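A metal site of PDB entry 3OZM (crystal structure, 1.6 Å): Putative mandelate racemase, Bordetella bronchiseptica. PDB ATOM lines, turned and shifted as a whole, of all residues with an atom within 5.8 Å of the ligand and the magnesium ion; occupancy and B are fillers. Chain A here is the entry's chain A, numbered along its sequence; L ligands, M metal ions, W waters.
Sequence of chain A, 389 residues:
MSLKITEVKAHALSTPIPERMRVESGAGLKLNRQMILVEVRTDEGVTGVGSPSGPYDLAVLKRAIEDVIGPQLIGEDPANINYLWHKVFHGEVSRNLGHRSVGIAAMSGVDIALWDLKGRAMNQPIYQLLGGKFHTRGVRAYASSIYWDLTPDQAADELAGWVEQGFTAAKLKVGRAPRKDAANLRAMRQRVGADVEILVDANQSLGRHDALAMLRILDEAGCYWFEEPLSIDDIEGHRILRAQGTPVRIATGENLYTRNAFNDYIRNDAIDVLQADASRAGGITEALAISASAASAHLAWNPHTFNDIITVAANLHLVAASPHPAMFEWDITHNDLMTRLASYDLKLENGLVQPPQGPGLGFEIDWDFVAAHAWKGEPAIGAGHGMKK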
ATOM      1  N   SER A  25     -10.263 -19.533  11.447  1.00  0.00           N
ATOM      2  CA  SER A  25      -9.371 -19.336  10.321  1.00  0.00           C
ATOM      3  C   SER A  25      -9.164 -20.697   9.662  1.00  0.00           C
ATOM      4  O   SER A  25      -9.855 -21.661   9.989  1.00  0.00           O
ATOM      5  CB  SER A  25      -8.019 -18.812  10.797  1.00  0.00           C
ATOM      6  OG  SER A  25      -7.396 -19.780  11.617  1.00  0.00           O
ATOM      7  N   GLY A  26      -8.210 -20.772   8.731  1.00  0.00           N
ATOM      8  CA  GLY A  26      -7.877 -22.038   8.109  1.00  0.00           C
ATOM      9  C   GLY A  26      -7.509 -23.109   9.121  1.00  0.00           C
ATOM     10  O   GLY A  26      -7.619 -24.301   8.836  1.00  0.00           O
ATOM     11  N   ALA A  27      -7.066 -22.683  10.307  1.00  0.00           N
ATOM     12  CA  ALA A  27      -6.658 -23.601  11.372  1.00  0.00           C
ATOM     13  C   ALA A  27      -7.848 -24.235  12.112  1.00  0.00           C
ATOM     14  O   ALA A  27      -7.678 -25.209  12.850  1.00  0.00           O
ATOM     15  CB  ALA A  27      -5.726 -22.889  12.372  1.00  0.00           C
ATOM     16  N   LYS A  30     -11.938 -21.779  16.924  1.00  0.00           N
ATOM     17  CA  LYS A  30     -11.468 -21.877  18.308  1.00  0.00           C
ATOM     18  C   LYS A  30     -12.629 -22.131  19.264  1.00  0.00           C
ATOM     19  O   LYS A  30     -13.700 -21.519  19.152  1.00  0.00           O
ATOM     20  CB  LYS A  30     -10.699 -20.613  18.716  1.00  0.00           C
ATOM     21  CG  LYS A  30      -9.490 -20.297  17.796  1.00  0.00           C
ATOM     22  CD  LYS A  30      -8.622 -19.158  18.348  1.00  0.00           C
ATOM     23  CE  LYS A  30      -7.650 -18.683  17.275  1.00  0.00           C
ATOM     24  NZ  LYS A  30      -6.821 -19.831  16.813  1.00  0.00           N
ATOM     25  N   GLY A  54       0.289 -24.666  21.054  1.00  0.00           N
ATOM     26  CA  GLY A  54      -0.935 -25.378  20.732  1.00  0.00           C
ATOM     27  C   GLY A  54      -1.525 -24.764  19.472  1.00  0.00           C
ATOM     28  O   GLY A  54      -0.987 -23.800  18.938  1.00  0.00           O
ATOM     29  N   PRO A  55      -2.648 -25.308  18.986  1.00  0.00           N
ATOM     30  CA  PRO A  55      -3.372 -26.459  19.529  1.00  0.00           C
ATOM     31  C   PRO A  55      -2.700 -27.781  19.195  1.00  0.00           C
ATOM     32  O   PRO A  55      -2.420 -28.084  18.013  1.00  0.00           O
ATOM     33  CB  PRO A  55      -4.735 -26.356  18.837  1.00  0.00           C
ATOM     34  CG  PRO A  55      -4.436 -25.681  17.543  1.00  0.00           C
ATOM     35  CD  PRO A  55      -3.371 -24.672  17.879  1.00  0.00           C
ATOM     36  N   TYR A 142       2.477  -6.490  16.367  1.00  0.00           N
ATOM     37  CA  TYR A 142       1.283  -6.449  15.531  1.00  0.00           C
ATOM     38  C   TYR A 142       0.111  -7.151  16.208  1.00  0.00           C
ATOM     39  O   TYR A 142       0.292  -8.120  16.958  1.00  0.00           O
ATOM     40  CB  TYR A 142       1.557  -6.978  14.110  1.00  0.00           C
ATOM     41  CG  TYR A 142       1.701  -8.486  13.930  1.00  0.00           C
ATOM     42  CD1 TYR A 142       0.578  -9.303  13.776  1.00  0.00           C
ATOM     43  CD2 TYR A 142       2.969  -9.080  13.860  1.00  0.00           C
ATOM     44  CE1 TYR A 142       0.711 -10.680  13.566  1.00  0.00           C
ATOM     45  CE2 TYR A 142       3.115 -10.440  13.655  1.00  0.00           C
ATOM     46  CZ  TYR A 142       1.991 -11.239  13.503  1.00  0.00           C
ATOM     47  OH  TYR A 142       2.132 -12.598  13.285  1.00  0.00           O
ATOM     48  N   SER A 144      -2.798  -9.570  16.323  1.00  0.00           N
ATOM     49  CA  SER A 144      -3.107 -10.841  15.675  1.00  0.00           C
ATOM     50  C   SER A 144      -4.402 -11.411  16.244  1.00  0.00           C
ATOM     51  O   SER A 144      -4.459 -11.741  17.431  1.00  0.00           O
ATOM     52  CB  SER A 144      -1.959 -11.810  15.963  1.00  0.00           C
ATOM     53  OG  SER A 144      -2.071 -13.007  15.220  1.00  0.00           O
ATOM     54  N   SER A 145      -5.461 -11.535  15.443  1.00  0.00           N
ATOM     55  CA  SER A 145      -5.555 -11.112  14.058  1.00  0.00           C
ATOM     56  C   SER A 145      -7.010 -10.745  13.852  1.00  0.00           C
ATOM     57  O   SER A 145      -7.839 -10.933  14.753  1.00  0.00           O
ATOM     58  CB  SER A 145      -5.250 -12.262  13.092  1.00  0.00           C
ATOM     59  OG  SER A 145      -3.883 -12.624  13.094  1.00  0.00           O
ATOM     60  N   TYR A 147     -10.149 -12.026  11.893  1.00  0.00           N
ATOM     61  CA  TYR A 147     -10.436 -13.384  11.430  1.00  0.00           C
ATOM     62  C   TYR A 147     -11.475 -13.457  10.310  1.00  0.00           C
ATOM     63  O   TYR A 147     -11.933 -12.426   9.817  1.00  0.00           O
ATOM     64  CB  TYR A 147     -10.831 -14.286  12.615  1.00  0.00           C
ATOM     65  CG  TYR A 147      -9.619 -14.809  13.352  1.00  0.00           C
ATOM     66  CD1 TYR A 147      -8.876 -13.981  14.189  1.00  0.00           C
ATOM     67  CD2 TYR A 147      -9.208 -16.124  13.192  1.00  0.00           C
ATOM     68  CE1 TYR A 147      -7.747 -14.460  14.843  1.00  0.00           C
ATOM     69  CE2 TYR A 147      -8.097 -16.611  13.858  1.00  0.00           C
ATOM     70  CZ  TYR A 147      -7.374 -15.777  14.686  1.00  0.00           C
ATOM     71  OH  TYR A 147      -6.256 -16.261  15.328  1.00  0.00           O
ATOM     72  N   LYS A 171      -2.779  -8.177  11.467  1.00  0.00           N
ATOM     73  CA  LYS A 171      -2.839  -9.298  10.530  1.00  0.00           C
ATOM     74  C   LYS A 171      -4.280  -9.722  10.222  1.00  0.00           C
ATOM     75  O   LYS A 171      -5.130  -9.743  11.129  1.00  0.00           O
ATOM     76  CB  LYS A 171      -2.049 -10.497  11.089  1.00  0.00           C
ATOM     77  CG  LYS A 171      -1.890 -11.640  10.092  1.00  0.00           C
ATOM     78  CD  LYS A 171      -0.704 -12.577  10.431  1.00  0.00           C
ATOM     79  CE  LYS A 171      -1.040 -13.554  11.592  1.00  0.00           C
ATOM     80  NZ  LYS A 171       0.189 -14.322  12.000  1.00  0.00           N
ATOM     81  N   LYS A 173      -6.733 -12.743   8.546  1.00  0.00           N
ATOM     82  CA  LYS A 173      -6.886 -14.113   8.103  1.00  0.00           C
ATOM     83  C   LYS A 173      -7.650 -14.184   6.783  1.00  0.00           C
ATOM     84  O   LYS A 173      -8.668 -13.496   6.595  1.00  0.00           O
ATOM     85  CB  LYS A 173      -7.598 -14.952   9.179  1.00  0.00           C
ATOM     86  CG  LYS A 173      -6.892 -14.920  10.505  1.00  0.00           C
ATOM     87  CD  LYS A 173      -5.558 -15.642  10.420  1.00  0.00           C
ATOM     88  CE  LYS A 173      -4.918 -15.724  11.792  1.00  0.00           C
ATOM     89  NZ  LYS A 173      -3.866 -16.771  11.828  1.00  0.00           N
ATOM     90  N   ASP A 201      -2.623 -13.772   6.351  1.00  0.00           N
ATOM     91  CA  ASP A 201      -2.318 -15.141   6.772  1.00  0.00           C
ATOM     92  C   ASP A 201      -3.386 -16.059   6.230  1.00  0.00           C
ATOM     93  O   ASP A 201      -4.555 -15.969   6.612  1.00  0.00           O
ATOM     94  CB  ASP A 201      -2.294 -15.211   8.305  1.00  0.00           C
ATOM     95  CG  ASP A 201      -1.843 -16.566   8.839  1.00  0.00           C
ATOM     96  OD1 ASP A 201      -1.738 -17.556   8.071  1.00  0.00           O
ATOM     97  OD2 ASP A 201      -1.593 -16.624  10.047  1.00  0.00           O
ATOM     98  N   ASN A 203      -3.220 -19.506   6.424  1.00  0.00           N
ATOM     99  CA  ASN A 203      -3.253 -20.788   7.106  1.00  0.00           C
ATOM    100  C   ASN A 203      -3.258 -22.005   6.167  1.00  0.00           C
ATOM    101  O   ASN A 203      -4.021 -22.948   6.369  1.00  0.00           O
ATOM    102  CB  ASN A 203      -4.466 -20.862   8.042  1.00  0.00           C
ATOM    103  CG  ASN A 203      -4.304 -19.948   9.242  1.00  0.00           C
ATOM    104  OD1 ASN A 203      -4.801 -18.820   9.249  1.00  0.00           O
ATOM    105  ND2 ASN A 203      -3.599 -20.431  10.257  1.00  0.00           N
ATOM    106  N   GLU A 227       1.537 -14.843   4.760  1.00  0.00           N
ATOM    107  CA  GLU A 227       1.902 -15.939   5.667  1.00  0.00           C
ATOM    108  C   GLU A 227       1.139 -17.218   5.352  1.00  0.00           C
ATOM    109  O   GLU A 227      -0.052 -17.194   5.069  1.00  0.00           O
ATOM    110  CB  GLU A 227       1.604 -15.501   7.109  1.00  0.00           C
ATOM    111  CG  GLU A 227       1.681 -16.616   8.152  1.00  0.00           C
ATOM    112  CD  GLU A 227       1.612 -16.063   9.566  1.00  0.00           C
ATOM    113  OE1 GLU A 227       1.684 -14.835   9.762  1.00  0.00           O
ATOM    114  OE2 GLU A 227       1.496 -16.887  10.498  1.00  0.00           O
ATOM    115  N   GLU A 228       1.849 -18.353   5.429  1.00  0.00           N
ATOM    116  CA  GLU A 228       1.328 -19.656   5.027  1.00  0.00           C
ATOM    117  C   GLU A 228       0.358 -19.577   3.840  1.00  0.00           C
ATOM    118  O   GLU A 228      -0.805 -19.987   3.940  1.00  0.00           O
ATOM    119  CB  GLU A 228       0.665 -20.386   6.209  1.00  0.00           C
ATOM    120  CG  GLU A 228       1.624 -20.876   7.319  1.00  0.00           C
ATOM    121  CD  GLU A 228       0.935 -21.886   8.263  1.00  0.00           C
ATOM    122  OE1 GLU A 228      -0.240 -21.654   8.622  1.00  0.00           O
ATOM    123  OE2 GLU A 228       1.561 -22.911   8.634  1.00  0.00           O
ATOM    124  N   GLU A 254       5.161 -21.447  11.391  1.00  0.00           N
ATOM    125  CA  GLU A 254       4.501 -21.941  12.593  1.00  0.00           C
ATOM    126  C   GLU A 254       4.286 -23.457  12.569  1.00  0.00           C
ATOM    127  O   GLU A 254       4.164 -24.090  13.616  1.00  0.00           O
ATOM    128  CB  GLU A 254       3.182 -21.216  12.822  1.00  0.00           C
ATOM    129  CG  GLU A 254       2.048 -21.713  11.989  1.00  0.00           C
ATOM    130  CD  GLU A 254       0.879 -20.752  12.054  1.00  0.00           C
ATOM    131  OE1 GLU A 254      -0.251 -21.159  12.374  1.00  0.00           O
ATOM    132  OE2 GLU A 254       1.116 -19.584  11.797  1.00  0.00           O
ATOM    133  N   GLN A 275       9.274 -17.995  10.396  1.00  0.00           N
ATOM    134  CA  GLN A 275       8.400 -17.770  11.546  1.00  0.00           C
ATOM    135  C   GLN A 275       8.513 -18.836  12.641  1.00  0.00           C
ATOM    136  O   GLN A 275       7.598 -18.995  13.444  1.00  0.00           O
ATOM    137  CB  GLN A 275       6.943 -17.608  11.079  1.00  0.00           C
ATOM    138  CG  GLN A 275       6.780 -16.377  10.161  1.00  0.00           C
ATOM    139  CD  GLN A 275       5.332 -16.150   9.742  1.00  0.00           C
ATOM    140  OE1 GLN A 275       4.729 -16.988   9.078  1.00  0.00           O
ATOM    141  NE2 GLN A 275       4.780 -15.006  10.115  1.00  0.00           N
ATOM    142  N   ARG A 280       7.489 -24.109  19.536  1.00  0.00           N
ATOM    143  CA  ARG A 280       7.019 -25.164  18.629  1.00  0.00           C
ATOM    144  C   ARG A 280       8.157 -25.841  17.888  1.00  0.00           C
ATOM    145  O   ARG A 280       8.190 -27.065  17.765  1.00  0.00           O
ATOM    146  CB  ARG A 280       6.015 -24.599  17.605  1.00  0.00           C
ATOM    147  CG  ARG A 280       4.771 -24.003  18.223  1.00  0.00           C
ATOM    148  CD  ARG A 280       3.959 -23.190  17.216  1.00  0.00           C
ATOM    149  NE  ARG A 280       3.281 -24.014  16.205  1.00  0.00           N
ATOM    150  CZ  ARG A 280       2.085 -24.563  16.399  1.00  0.00           C
ATOM    151  NH1 ARG A 280       1.443 -24.388  17.557  1.00  0.00           N
ATOM    152  NH2 ARG A 280       1.508 -25.275  15.435  1.00  0.00           N
ATOM    153  N   HIS A 304       6.248 -16.812  14.903  1.00  0.00           N
ATOM    154  CA  HIS A 304       4.900 -17.079  15.381  1.00  0.00           C
ATOM    155  C   HIS A 304       4.981 -17.152  16.919  1.00  0.00           C
ATOM    156  O   HIS A 304       5.972 -17.685  17.461  1.00  0.00           O
ATOM    157  CB  HIS A 304       4.426 -18.406  14.792  1.00  0.00           C
ATOM    158  CG  HIS A 304       3.128 -18.912  15.360  1.00  0.00           C
ATOM    159  ND1 HIS A 304       3.059 -19.674  16.505  1.00  0.00           N
ATOM    160  CD2 HIS A 304       1.852 -18.787  14.903  1.00  0.00           C
ATOM    161  CE1 HIS A 304       1.795 -19.992  16.739  1.00  0.00           C
ATOM    162  NE2 HIS A 304       1.047 -19.477  15.776  1.00  0.00           N
ATOM    163  N   THR A 305       3.983 -16.619  17.614  1.00  0.00           N
ATOM    164  CA  THR A 305       4.019 -16.577  19.087  1.00  0.00           C
ATOM    165  C   THR A 305       2.684 -16.989  19.732  1.00  0.00           C
ATOM    166  O   THR A 305       2.554 -16.973  20.963  1.00  0.00           O
ATOM    167  CB  THR A 305       4.312 -15.166  19.603  1.00  0.00           C
ATOM    168  OG1 THR A 305       3.159 -14.323  19.409  1.00  0.00           O
ATOM    169  CG2 THR A 305       5.536 -14.555  18.933  1.00  0.00           C
ATOM    170  N   PHE A 306       1.726 -17.390  18.915  1.00  0.00           N
ATOM    171  CA  PHE A 306       0.304 -17.459  19.284  1.00  0.00           C
ATOM    172  C   PHE A 306      -0.098 -18.720  20.069  1.00  0.00           C
ATOM    173  O   PHE A 306      -0.173 -19.818  19.516  1.00  0.00           O
ATOM    174  CB  PHE A 306      -0.498 -17.358  17.975  1.00  0.00           C
ATOM    175  CG  PHE A 306      -1.953 -16.980  18.118  1.00  0.00           C
ATOM    176  CD1 PHE A 306      -2.367 -15.655  17.941  1.00  0.00           C
ATOM    177  CD2 PHE A 306      -2.920 -17.948  18.327  1.00  0.00           C
ATOM    178  CE1 PHE A 306      -3.707 -15.304  18.011  1.00  0.00           C
ATOM    179  CE2 PHE A 306      -4.278 -17.605  18.409  1.00  0.00           C
ATOM    180  CZ  PHE A 306      -4.666 -16.290  18.245  1.00  0.00           C
ATOM    181  N   GLU A 329       4.290 -10.772  16.905  1.00  0.00           N
ATOM    182  CA  GLU A 329       2.894 -11.197  16.976  1.00  0.00           C
ATOM    183  C   GLU A 329       2.345 -11.096  18.389  1.00  0.00           C
ATOM    184  O   GLU A 329       2.906 -11.684  19.320  1.00  0.00           O
ATOM    185  CB  GLU A 329       2.743 -12.643  16.481  1.00  0.00           C
ATOM    186  CG  GLU A 329       1.289 -13.116  16.469  1.00  0.00           C
ATOM    187  CD  GLU A 329       1.088 -14.454  15.806  1.00  0.00           C
ATOM    188  OE1 GLU A 329       2.005 -15.299  15.833  1.00  0.00           O
ATOM    189  OE2 GLU A 329      -0.034 -14.668  15.275  1.00  0.00           O
ATOM    190  N   ILE A 381     -10.134 -26.794  19.480  1.00  0.00           N
ATOM    191  CA  ILE A 381     -10.383 -26.201  18.169  1.00  0.00           C
ATOM    192  C   ILE A 381     -11.129 -27.181  17.276  1.00  0.00           C
ATOM    193  O   ILE A 381     -10.933 -28.396  17.380  1.00  0.00           O
ATOM    194  CB  ILE A 381      -9.054 -25.733  17.537  1.00  0.00           C
ATOM    195  CG1 ILE A 381      -9.291 -24.798  16.342  1.00  0.00           C
ATOM    196  CG2 ILE A 381      -8.158 -26.904  17.165  1.00  0.00           C
ATOM    197  CD1 ILE A 381      -8.026 -24.042  15.931  1.00  0.00           C
HETATM  198  O1  LIG L   1      -5.527 -18.660  14.758  1.00  0.00           O
HETATM  199  O2  LIG L   1      -4.086 -20.809  15.605  1.00  0.00           O
HETATM  200  O3  LIG L   1      -1.970 -18.980  12.262  1.00  0.00           O
HETATM  201  O4  LIG L   1      -1.098 -16.826  15.025  1.00  0.00           O
HETATM  202  O5  LIG L   1      -5.029 -19.187  12.665  1.00  0.00           O
HETATM  203  C1  LIG L   1      -4.853 -19.259  13.909  1.00  0.00           C
HETATM  204  C2  LIG L   1      -3.704 -20.149  14.388  1.00  0.00           C
HETATM  205  C3  LIG L   1      -2.462 -19.281  14.674  1.00  0.00           C
HETATM  206  C4  LIG L   1      -2.191 -18.308  13.510  1.00  0.00           C
HETATM  207  C5  LIG L   1      -1.122 -17.240  13.849  1.00  0.00           C
HETATM  208  O6  LIG L   1      -0.355 -16.828  12.934  1.00  0.00           O
HETATM  209  O7  LIG L   1      -1.356 -20.137  14.970  1.00  0.00           O
HETATM  210 MG    MG M   1      -0.275 -18.080  11.094  1.00  0.00          MG
HETATM  211  O   HOH W   1      -8.135 -20.633  14.335  1.00  0.00           O
HETATM  212  O   HOH W   2       2.766 -16.034  12.853  1.00  0.00           O
HETATM  213  O   HOH W   3      -0.497 -19.403   9.484  1.00  0.00           O
HETATM  214  O   HOH W   4      -3.749 -15.129  14.621  1.00  0.00           O
HETATM  215  O   HOH W   5      -1.888 -21.553  17.955  1.00  0.00           O
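OE2 of Glu 329 sits close to O4 of the ligand, 2.4 Å away.
O1 of the ligand is in hydrogen-bond range of OH of Tyr 147, 2.6 Å away.
A ring nitrogen (NE2) of His 304 lies within hydrogen-bond range of an oxygen (O7) of the ligand (2.6 Å).
The side-chain hydroxyl of Ser 25 sits at hydrogen-bond distance from an oxygen (O5) of the ligand (2.7 Å).
The side-chain amino group (NZ) of Lys 30 lies within salt-bridge range of an oxygen (O1) of the ligand.
An oxygen (O6) of the ligand lies close to the side-chain amino group of Lys 171 (2.7 Å).
The side-chain amino group (NZ) of Lys 173 lies within salt-bridge range of an oxygen (O5) of the ligand.
An oxygen (O5) of the ligand sits at hydrogen-bond distance from the side-chain amide nitrogen (ND2) of Asn 203.
OE1 of Glu 227 is in salt-bridge range of NZ of Lys 171 (2.7 Å).
NE2 of Gln 275 lies within hydrogen-bond range of OE1 of Glu 227 (3.1 Å).
The side-chain carboxylate (OD2) of Asp 201 lies close to the side-chain amino group (NZ) of Lys 171, 3.5 Å away.
N of Asn 203 sits at hydrogen-bond distance from OD1 of Asp 201 (3.0 Å).
OE2 of Glu 329 is in salt-bridge range of NZ of Lys 171.
OE2 of Glu 329 lies within hydrogen-bond range of OG of Ser 144, 2.6 Å away.
The side-chain hydroxyl of Thr 305 is in hydrogen-bond range of the backbone carbonyl oxygen of Glu 329.
The backbone carbonyl oxygen of Gln 275 is in hydrogen-bond range of the backbone NH of His 304, at 3.0 Å.
Residues that only touch the ligand: Phe 306 (3.1 Å), Ala 27 (3.8 Å) and Ser 144 (3.9 Å).
Hydrophobic or aromatic side chains that line the ligand: Ala 27, Tyr 147, His 304 and Phe 306.
Within 4 Å of the ligand: Ser 25, Ala 27, Lys 30, Ser 144, Tyr 147, Lys 171, Lys 173, Asp 201, Asn 203, Glu 227, Glu 254, His 304, Phe 306 and Glu 329.
The nearest printed residue that does not touch the ligand is Pro 55 (4.5 Å).
Merely in contact with the magnesium ion: Lys 171 and Lys 173.
Five residues have an atom within 4 Å of the magnesium ion: Lys 171, Lys 173, Asp 201, Glu 227 and Glu 254.
The nearest printed residue that does not touch the magnesium ion is Asn 203 (4.2 Å).
The magnesium ion is bound by water W3 (2.1 Å), the side-chain carboxylate (OE2) of Glu 254 (2.2 Å), the side-chain carboxylate (OE2) of Glu 227 (2.2 Å), the side-chain carboxylate (OD2) of Asp 201 (2.2 Å), an oxygen (O6) of the ligand (2.2 Å) and an oxygen (O3) of the ligand (2.2 Å).
The magnesium ion has six donor atoms within binding distance.
Water W4 lies within hydrogen-bond range of OG of Ser 144 (2.8 Å), OH of Tyr 147 (2.8 Å), OG of Ser 145 (2.9 Å), O4 of the ligand (3.2 Å) and NZ of Lys 173 (3.2 Å).
Water W2 lies within hydrogen-bond range of the side-chain carboxylate (OE1) of Glu 329, the side-chain amino group (NZ) of Lys 171 and the side-chain carboxylate (OE1) of Glu 227.
Water W1 lies within hydrogen-bond range of NZ of Lys 30 (2.9 Å), OG of Ser 25 (2.9 Å) and O1 of the ligand (3.3 Å).
Water W5 lies within hydrogen-bond range of the backbone carbonyl oxygen of Gly 54 (2.6 Å), the backbone carbonyl oxygen of Phe 306 (2.9 Å) and an oxygen (O2) of the ligand (3.3 Å).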
